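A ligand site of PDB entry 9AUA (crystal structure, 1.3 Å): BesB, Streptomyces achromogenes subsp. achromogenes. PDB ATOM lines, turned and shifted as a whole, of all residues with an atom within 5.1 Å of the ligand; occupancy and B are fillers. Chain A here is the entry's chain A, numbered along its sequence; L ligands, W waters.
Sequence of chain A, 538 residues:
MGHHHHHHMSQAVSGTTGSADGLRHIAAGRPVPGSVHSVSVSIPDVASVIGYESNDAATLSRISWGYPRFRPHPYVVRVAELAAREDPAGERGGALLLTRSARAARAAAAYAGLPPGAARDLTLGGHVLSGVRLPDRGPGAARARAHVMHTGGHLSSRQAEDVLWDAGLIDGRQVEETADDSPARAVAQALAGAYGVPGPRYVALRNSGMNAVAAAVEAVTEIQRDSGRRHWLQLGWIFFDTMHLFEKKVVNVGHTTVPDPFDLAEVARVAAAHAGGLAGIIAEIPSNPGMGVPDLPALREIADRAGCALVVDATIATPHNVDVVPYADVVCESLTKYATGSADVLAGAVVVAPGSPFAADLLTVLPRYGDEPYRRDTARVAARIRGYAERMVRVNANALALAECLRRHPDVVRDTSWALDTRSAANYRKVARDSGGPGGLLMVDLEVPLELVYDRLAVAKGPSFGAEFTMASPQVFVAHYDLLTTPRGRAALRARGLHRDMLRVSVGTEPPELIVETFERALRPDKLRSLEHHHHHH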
ATOM      1  N   TYR A  67      17.453   5.521  16.184  1.00  0.00           N
ATOM      2  CA  TYR A  67      18.849   5.390  15.793  1.00  0.00           C
ATOM      3  C   TYR A  67      19.615   4.754  16.942  1.00  0.00           C
ATOM      4  O   TYR A  67      19.416   5.143  18.101  1.00  0.00           O
ATOM      5  CB  TYR A  67      19.387   6.797  15.506  1.00  0.00           C
ATOM      6  CG  TYR A  67      20.713   6.805  14.799  1.00  0.00           C
ATOM      7  CD1 TYR A  67      20.816   6.444  13.456  1.00  0.00           C
ATOM      8  CD2 TYR A  67      21.869   7.169  15.482  1.00  0.00           C
ATOM      9  CE1 TYR A  67      22.034   6.454  12.811  1.00  0.00           C
ATOM     10  CE2 TYR A  67      23.104   7.178  14.841  1.00  0.00           C
ATOM     11  CZ  TYR A  67      23.180   6.821  13.508  1.00  0.00           C
ATOM     12  OH  TYR A  67      24.378   6.820  12.828  1.00  0.00           O
ATOM     13  N   ARG A  69      22.473   4.781  18.440  1.00  0.00           N
ATOM     14  CA  ARG A  69      23.204   5.540  19.452  1.00  0.00           C
ATOM     15  C   ARG A  69      22.269   6.334  20.364  1.00  0.00           C
ATOM     16  O   ARG A  69      22.701   6.756  21.447  1.00  0.00           O
ATOM     17  CB  ARG A  69      24.202   6.506  18.808  1.00  0.00           C
ATOM     18  CG  ARG A  69      25.292   5.796  18.019  1.00  0.00           C
ATOM     19  CD  ARG A  69      26.505   6.694  17.768  1.00  0.00           C
ATOM     20  NE  ARG A  69      26.187   7.785  16.852  1.00  0.00           N
ATOM     21  CZ  ARG A  69      25.937   9.022  17.224  1.00  0.00           C
ATOM     22  NH1 ARG A  69      25.967   9.360  18.521  1.00  0.00           N
ATOM     23  NH2 ARG A  69      25.645   9.945  16.312  1.00  0.00           N
ATOM     24  N   SER A 208      31.744   3.667  14.918  1.00  0.00           N
ATOM     25  CA  SER A 208      30.748   4.519  14.265  1.00  0.00           C
ATOM     26  C   SER A 208      31.487   5.768  13.828  1.00  0.00           C
ATOM     27  O   SER A 208      32.677   5.935  14.118  1.00  0.00           O
ATOM     28  CB  SER A 208      29.555   4.826  15.201  1.00  0.00           C
ATOM     29  OG  SER A 208      29.889   5.899  16.068  1.00  0.00           O
ATOM     30  N   GLY A 209      30.795   6.639  13.103  1.00  0.00           N
ATOM     31  CA  GLY A 209      31.396   7.916  12.735  1.00  0.00           C
ATOM     32  C   GLY A 209      31.908   8.677  13.945  1.00  0.00           C
ATOM     33  O   GLY A 209      33.013   9.218  13.934  1.00  0.00           O
ATOM     34  N   MET A 210      31.089   8.755  15.001  1.00  0.00           N
ATOM     35  CA  MET A 210      31.511   9.465  16.197  1.00  0.00           C
ATOM     36  C   MET A 210      32.687   8.788  16.889  1.00  0.00           C
ATOM     37  O   MET A 210      33.507   9.478  17.489  1.00  0.00           O
ATOM     38  CB  MET A 210      30.358   9.583  17.188  1.00  0.00           C
ATOM     39  CG  MET A 210      29.292  10.609  16.816  1.00  0.00           C
ATOM     40  SD  MET A 210      29.949  12.172  16.184  1.00  0.00           S
ATOM     41  CE  MET A 210      31.055  12.665  17.512  1.00  0.00           C
ATOM     42  N   ASN A 211      32.764   7.461  16.830  1.00  0.00           N
ATOM     43  CA  ASN A 211      33.915   6.793  17.400  1.00  0.00           C
ATOM     44  C   ASN A 211      35.177   7.160  16.635  1.00  0.00           C
ATOM     45  O   ASN A 211      36.258   7.294  17.238  1.00  0.00           O
ATOM     46  CB  ASN A 211      33.670   5.288  17.399  1.00  0.00           C
ATOM     47  CG  ASN A 211      34.556   4.547  18.400  1.00  0.00           C
ATOM     48  OD1 ASN A 211      35.405   3.734  18.017  1.00  0.00           O
ATOM     49  ND2 ASN A 211      34.342   4.810  19.690  1.00  0.00           N
ATOM     50  N   VAL A 213      35.592  10.135  14.949  1.00  0.00           N
ATOM     51  CA  VAL A 213      35.866  11.528  15.310  1.00  0.00           C
ATOM     52  C   VAL A 213      36.518  11.611  16.692  1.00  0.00           C
ATOM     53  O   VAL A 213      37.527  12.293  16.879  1.00  0.00           O
ATOM     54  CB  VAL A 213      34.582  12.381  15.247  1.00  0.00           C
ATOM     55  CG1 VAL A 213      34.818  13.782  15.825  1.00  0.00           C
ATOM     56  CG2 VAL A 213      34.097  12.475  13.822  1.00  0.00           C
ATOM     57  N   PHE A 239      28.276  18.817  13.491  1.00  0.00           N
ATOM     58  CA  PHE A 239      27.347  17.798  13.965  1.00  0.00           C
ATOM     59  C   PHE A 239      27.257  17.822  15.490  1.00  0.00           C
ATOM     60  O   PHE A 239      28.265  17.965  16.183  1.00  0.00           O
ATOM     61  CB  PHE A 239      27.786  16.414  13.490  1.00  0.00           C
ATOM     62  CG  PHE A 239      26.867  15.331  13.938  1.00  0.00           C
ATOM     63  CD1 PHE A 239      25.513  15.382  13.636  1.00  0.00           C
ATOM     64  CD2 PHE A 239      27.349  14.289  14.711  1.00  0.00           C
ATOM     65  CE1 PHE A 239      24.651  14.392  14.071  1.00  0.00           C
ATOM     66  CE2 PHE A 239      26.499  13.283  15.144  1.00  0.00           C
ATOM     67  CZ  PHE A 239      25.149  13.339  14.829  1.00  0.00           C
ATOM     68  N   THR A 242      29.555  15.860  17.805  1.00  0.00           N
ATOM     69  CA  THR A 242      30.911  16.370  17.813  1.00  0.00           C
ATOM     70  C   THR A 242      31.024  17.606  18.686  1.00  0.00           C
ATOM     71  O   THR A 242      31.995  17.751  19.446  1.00  0.00           O
ATOM     72  CB  THR A 242      31.361  16.669  16.379  1.00  0.00           C
ATOM     73  OG1 THR A 242      31.193  15.483  15.585  1.00  0.00           O
ATOM     74  CG2 THR A 242      32.823  17.123  16.345  1.00  0.00           C
ATOM     75  N   GLU A 284      33.971  20.498   9.214  1.00  0.00           N
ATOM     76  CA  GLU A 284      33.166  19.570   8.426  1.00  0.00           C
ATOM     77  C   GLU A 284      33.024  20.097   7.008  1.00  0.00           C
ATOM     78  O   GLU A 284      33.037  21.314   6.790  1.00  0.00           O
ATOM     79  CB  GLU A 284      31.760  19.410   9.001  1.00  0.00           C
ATOM     80  CG  GLU A 284      31.714  18.650  10.296  1.00  0.00           C
ATOM     81  CD  GLU A 284      30.322  18.528  10.849  1.00  0.00           C
ATOM     82  OE1 GLU A 284      29.429  19.321  10.456  1.00  0.00           O
ATOM     83  OE2 GLU A 284      30.107  17.676  11.725  1.00  0.00           O
ATOM     84  N   ASN A 288      26.982  19.754   9.151  1.00  0.00           N
ATOM     85  CA  ASN A 288      25.694  19.152   9.475  1.00  0.00           C
ATOM     86  C   ASN A 288      25.018  19.990  10.544  1.00  0.00           C
ATOM     87  O   ASN A 288      25.557  20.101  11.651  1.00  0.00           O
ATOM     88  CB  ASN A 288      25.915  17.731   9.988  1.00  0.00           C
ATOM     89  CG  ASN A 288      24.613  16.932  10.130  1.00  0.00           C
ATOM     90  OD1 ASN A 288      23.511  17.497  10.147  1.00  0.00           O
ATOM     91  ND2 ASN A 288      24.733  15.615  10.236  1.00  0.00           N
ATOM     92  N   ASP A 313      35.878  16.330   8.831  1.00  0.00           N
ATOM     93  CA  ASP A 313      34.850  15.293   8.699  1.00  0.00           C
ATOM     94  C   ASP A 313      34.170  15.531   7.359  1.00  0.00           C
ATOM     95  O   ASP A 313      33.425  16.502   7.198  1.00  0.00           O
ATOM     96  CB  ASP A 313      33.868  15.387   9.867  1.00  0.00           C
ATOM     97  CG  ASP A 313      32.803  14.322   9.839  1.00  0.00           C
ATOM     98  OD1 ASP A 313      32.508  13.776   8.755  1.00  0.00           O
ATOM     99  OD2 ASP A 313      32.250  14.043  10.921  1.00  0.00           O
ATOM    100  N   THR A 315      32.081  13.419   5.748  1.00  0.00           N
ATOM    101  CA  THR A 315      30.950  12.513   5.561  1.00  0.00           C
ATOM    102  C   THR A 315      29.951  13.015   4.528  1.00  0.00           C
ATOM    103  O   THR A 315      29.505  12.258   3.658  1.00  0.00           O
ATOM    104  CB  THR A 315      30.239  12.334   6.903  1.00  0.00           C
ATOM    105  OG1 THR A 315      31.141  11.715   7.827  1.00  0.00           O
ATOM    106  CG2 THR A 315      28.985  11.470   6.756  1.00  0.00           C
ATOM    107  N   ILE A 316      29.570  14.290   4.631  1.00  0.00           N
ATOM    108  CA  ILE A 316      28.463  14.762   3.803  1.00  0.00           C
ATOM    109  C   ILE A 316      28.870  14.946   2.347  1.00  0.00           C
ATOM    110  O   ILE A 316      28.036  14.782   1.442  1.00  0.00           O
ATOM    111  CB  ILE A 316      27.824  16.003   4.447  1.00  0.00           C
ATOM    112  CG1 ILE A 316      27.188  15.596   5.771  1.00  0.00           C
ATOM    113  CG2 ILE A 316      26.792  16.643   3.514  1.00  0.00           C
ATOM    114  CD1 ILE A 316      26.696  16.783   6.605  1.00  0.00           C
ATOM    115  N   SER A 334      31.702   9.031   8.682  1.00  0.00           N
ATOM    116  CA  SER A 334      30.699   8.074   9.132  1.00  0.00           C
ATOM    117  C   SER A 334      30.303   7.179   7.973  1.00  0.00           C
ATOM    118  O   SER A 334      29.599   7.619   7.054  1.00  0.00           O
ATOM    119  CB  SER A 334      29.459   8.813   9.628  1.00  0.00           C
ATOM    120  OG  SER A 334      28.486   7.840   9.973  1.00  0.00           O
ATOM    121  N   THR A 336      28.280   4.844   8.175  1.00  0.00           N
ATOM    122  CA  THR A 336      26.850   4.593   8.352  1.00  0.00           C
ATOM    123  C   THR A 336      26.029   5.188   7.218  1.00  0.00           C
ATOM    124  O   THR A 336      24.920   4.718   6.941  1.00  0.00           O
ATOM    125  CB  THR A 336      26.440   5.270   9.657  1.00  0.00           C
ATOM    126  OG1 THR A 336      27.374   4.883  10.688  1.00  0.00           O
ATOM    127  CG2 THR A 336      25.003   4.910  10.067  1.00  0.00           C
ATOM    128  N   LYS A 337      26.543   6.238   6.581  1.00  0.00           N
ATOM    129  CA  LYS A 337      25.797   7.026   5.608  1.00  0.00           C
ATOM    130  C   LYS A 337      26.039   6.501   4.204  1.00  0.00           C
ATOM    131  O   LYS A 337      25.885   5.290   3.967  1.00  0.00           O
ATOM    132  CB  LYS A 337      26.128   8.507   5.806  1.00  0.00           C
ATOM    133  CG  LYS A 337      26.125   8.920   7.298  1.00  0.00           C
ATOM    134  CD  LYS A 337      24.811   8.659   8.014  1.00  0.00           C
ATOM    135  CE  LYS A 337      24.950   9.054   9.488  1.00  0.00           C
ATOM    136  NZ  LYS A 337      23.795   8.631  10.329  1.00  0.00           N
ATOM    137  N   LEU A 346      26.404   0.766  11.469  1.00  0.00           N
ATOM    138  CA  LEU A 346      27.236   1.872  11.900  1.00  0.00           C
ATOM    139  C   LEU A 346      28.707   1.483  11.808  1.00  0.00           C
ATOM    140  O   LEU A 346      29.097   0.378  12.172  1.00  0.00           O
ATOM    141  CB  LEU A 346      26.936   2.301  13.338  1.00  0.00           C
ATOM    142  CG  LEU A 346      25.814   3.332  13.481  1.00  0.00           C
ATOM    143  CD1 LEU A 346      24.478   2.718  13.147  1.00  0.00           C
ATOM    144  CD2 LEU A 346      25.790   3.891  14.885  1.00  0.00           C
ATOM    145  N   ALA A 347      29.518   2.409  11.304  1.00  0.00           N
ATOM    146  CA  ALA A 347      30.975   2.271  11.311  1.00  0.00           C
ATOM    147  C   ALA A 347      31.558   3.632  10.959  1.00  0.00           C
ATOM    148  O   ALA A 347      30.903   4.477  10.353  1.00  0.00           O
ATOM    149  CB  ALA A 347      31.468   1.205  10.309  1.00  0.00           C
ATOM    150  N   PRO A 463      15.281   9.569  11.284  1.00  0.00           N
ATOM    151  CA  PRO A 463      16.691   9.899  11.534  1.00  0.00           C
ATOM    152  C   PRO A 463      17.658   9.248  10.557  1.00  0.00           C
ATOM    153  O   PRO A 463      17.327   8.294   9.834  1.00  0.00           O
ATOM    154  CB  PRO A 463      16.929   9.392  12.957  1.00  0.00           C
ATOM    155  CG  PRO A 463      15.920   8.302  13.149  1.00  0.00           C
ATOM    156  CD  PRO A 463      14.717   8.691  12.325  1.00  0.00           C
ATOM    157  N   SER A 464      18.877   9.784  10.548  1.00  0.00           N
ATOM    158  CA  SER A 464      19.990   9.371   9.698  1.00  0.00           C
ATOM    159  C   SER A 464      19.832   9.875   8.267  1.00  0.00           C
ATOM    160  O   SER A 464      18.921  10.668   7.978  1.00  0.00           O
ATOM    161  CB  SER A 464      20.250   7.850   9.760  1.00  0.00           C
ATOM    162  OG  SER A 464      21.572   7.534   9.337  1.00  0.00           O
ATOM    163  N   PHE A 465      20.736   9.475   7.397  1.00  0.00           N
ATOM    164  CA  PHE A 465      20.750   9.901   5.999  1.00  0.00           C
ATOM    165  C   PHE A 465      21.677   8.956   5.250  1.00  0.00           C
ATOM    166  O   PHE A 465      22.297   8.062   5.844  1.00  0.00           O
ATOM    167  CB  PHE A 465      21.173  11.371   5.832  1.00  0.00           C
ATOM    168  CG  PHE A 465      22.601  11.696   6.226  1.00  0.00           C
ATOM    169  CD1 PHE A 465      23.660  11.611   5.319  1.00  0.00           C
ATOM    170  CD2 PHE A 465      22.890  12.162   7.506  1.00  0.00           C
ATOM    171  CE1 PHE A 465      24.955  11.968   5.683  1.00  0.00           C
ATOM    172  CE2 PHE A 465      24.178  12.526   7.871  1.00  0.00           C
ATOM    173  CZ  PHE A 465      25.212  12.423   6.966  1.00  0.00           C
ATOM    174  N   GLN A 475      15.438  18.044  10.929  1.00  0.00           N
ATOM    175  CA  GLN A 475      16.715  17.899  11.627  1.00  0.00           C
ATOM    176  C   GLN A 475      16.890  18.882  12.780  1.00  0.00           C
ATOM    177  O   GLN A 475      17.646  18.576  13.715  1.00  0.00           O
ATOM    178  CB  GLN A 475      17.878  17.961  10.639  1.00  0.00           C
ATOM    179  CG  GLN A 475      19.255  17.581  11.215  1.00  0.00           C
ATOM    180  CD  GLN A 475      19.330  16.148  11.774  1.00  0.00           C
ATOM    181  OE1 GLN A 475      18.480  15.293  11.519  1.00  0.00           O
ATOM    182  NE2 GLN A 475      20.386  15.882  12.549  1.00  0.00           N
ATOM    183  N   ARG A 504      15.878  18.482   6.242  1.00  0.00           N
ATOM    184  CA  ARG A 504      17.109  18.022   5.647  1.00  0.00           C
ATOM    185  C   ARG A 504      16.779  16.859   4.726  1.00  0.00           C
ATOM    186  O   ARG A 504      16.356  15.797   5.192  1.00  0.00           O
ATOM    187  CB  ARG A 504      18.101  17.585   6.717  1.00  0.00           C
ATOM    188  CG  ARG A 504      19.417  17.100   6.115  1.00  0.00           C
ATOM    189  CD  ARG A 504      20.329  16.485   7.153  1.00  0.00           C
ATOM    190  NE  ARG A 504      19.835  15.179   7.582  1.00  0.00           N
ATOM    191  CZ  ARG A 504      20.296  14.545   8.639  1.00  0.00           C
ATOM    192  NH1 ARG A 504      21.271  15.096   9.363  1.00  0.00           N
ATOM    193  NH2 ARG A 504      19.813  13.358   8.973  1.00  0.00           N
HETATM  194  C1  LIG L   1      29.099  14.784   9.618  1.00  0.00           C
HETATM  195  O1  LIG L   1      22.502  13.718  11.175  1.00  0.00           O
HETATM  196  O2  LIG L   1      23.260  10.627  12.454  1.00  0.00           O
HETATM  197  O3  LIG L   1      26.208   7.979  13.925  1.00  0.00           O
HETATM  198  O4  LIG L   1      21.210  11.956  11.038  1.00  0.00           O
HETATM  199  O5  LIG L   1      26.557  13.755   9.971  1.00  0.00           O
HETATM  200  O6  LIG L   1      28.522   7.877  14.814  1.00  0.00           O
HETATM  201  O7  LIG L   1      28.005   6.769  12.601  1.00  0.00           O
HETATM  202  C2  LIG L   1      24.846  12.180  11.619  1.00  0.00           C
HETATM  203  C3  LIG L   1      25.937  11.498  11.869  1.00  0.00           C
HETATM  204  C4  LIG L   1      29.668  12.144  12.119  1.00  0.00           C
HETATM  205  C5  LIG L   1      28.240  10.458  13.323  1.00  0.00           C
HETATM  206  N1  LIG L   1      29.861  13.125  11.266  1.00  0.00           N
HETATM  207  O8  LIG L   1      28.104   9.211  12.698  1.00  0.00           O
HETATM  208  C6  LIG L   1      22.312  12.480  11.332  1.00  0.00           C
HETATM  209  C7  LIG L   1      23.451  11.635  11.867  1.00  0.00           C
HETATM  210  C8  LIG L   1      28.850  13.635  10.591  1.00  0.00           C
HETATM  211  C9  LIG L   1      27.560  13.153  10.737  1.00  0.00           C
HETATM  212  C10 LIG L   1      28.400  11.597  12.321  1.00  0.00           C
HETATM  213  C11 LIG L   1      27.313  12.104  11.620  1.00  0.00           C
HETATM  214  P1  LIG L   1      27.692   7.882  13.573  1.00  0.00           P
HETATM  215  O   HOH W   1      18.988  12.417  12.033  1.00  0.00           O
HETATM  216  O   HOH W   2      20.967   9.784  13.237  1.00  0.00           O
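NE2 of Gln 475 is in hydrogen-bond range of O1 of the ligand, at 3.3 Å. The side-chain hydroxyl (OG) of Ser 334 sits at hydrogen-bond distance from an oxygen (O7) of the ligand (2.9 Å). An oxygen (O6) of the ligand sits at hydrogen-bond distance from the backbone NH of Met 210 (2.7 Å). NZ of Lys 337 sits at hydrogen-bond distance from O2 of the ligand (3.0 Å). An oxygen (O7) of the ligand is in hydrogen-bond range of the side-chain hydroxyl of Thr 336, at 2.8 Å. The backbone NH (N) of Ser 464 sits close to an oxygen (O4) of the ligand. N1 of the ligand lies within hydrogen-bond range of OD2 of Asp 313, at 2.6 Å. The guanidinium group of Arg 69 lies within salt-bridge range of an oxygen (O3) of the ligand. An oxygen (O5) of the ligand is in hydrogen-bond range of the side-chain amide nitrogen (ND2) of Asn 288 (2.6 Å). O6 of the ligand is in hydrogen-bond range of OG of Ser 208 (2.7 Å). O7 of the ligand is in hydrogen-bond range of N of Gly 209 (2.8 Å). The guanidinium group (NH1) of Arg 504 is in salt-bridge range of an oxygen (O1) of the ligand (2.6 Å). The side-chain hydroxyl (OH) of Tyr 67 is in hydrogen-bond range of an oxygen (O3) of the ligand, at 2.4 Å.
NH1 of Arg 504 sits at hydrogen-bond distance from OD1 of Asn 288, at 3.4 Å. The side-chain amino group (NZ) of Lys 337 lies within hydrogen-bond range of the side-chain hydroxyl (OG) of Ser 464 (2.7 Å). OE2 of Glu 284 is in hydrogen-bond range of N of Phe 239 (2.8 Å). The side-chain hydroxyl (OG1) of Thr 336 lies within hydrogen-bond range of the side-chain hydroxyl (OG) of Ser 334 (3.2 Å). The side-chain hydroxyl (OH) of Tyr 67 is in hydrogen-bond range of the side-chain amino group (NZ) of Lys 337. The backbone carbonyl oxygen (O) of Ala 347 is in hydrogen-bond range of the backbone NH (N) of Gly 209 (3.5 Å). OG1 of Thr 336 lies within hydrogen-bond range of N of Ala 347, 3.3 Å away. The guanidinium group (NH1) of Arg 504 lies close to the side-chain amide nitrogen (NE2) of Gln 475.
Merely in contact with the ligand: Phe 239 (3.3 Å), Phe 465 (3.4 Å), Glu 284 (3.7 Å) and Thr 315 (3.8 Å). Hydrophobic or aromatic side chains within 4 Å of the ligand: Tyr 67, Met 210, Phe 239 and Phe 465. Within 4 Å of the ligand: Tyr 67, Arg 69, Ser 208, Gly 209, Met 210, Phe 239, Glu 284, Asn 288, Asp 313, Thr 315, Ser 334, Thr 336, Lys 337, Ser 464, Phe 465, Gln 475 and Arg 504. The nearest printed residue that does not touch the ligand is Leu 346 (4.2 Å).
Water W1 lies within hydrogen-bond range of O4 of the ligand (2.5 Å), OE1 of Gln 475 (3.0 Å), N of Ser 464 (3.0 Å) and NH2 of Arg 504 (3.3 Å). Water W2 lies within hydrogen-bond range of O2 of the ligand (2.6 Å) and N of Ser 464 (3.4 Å).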
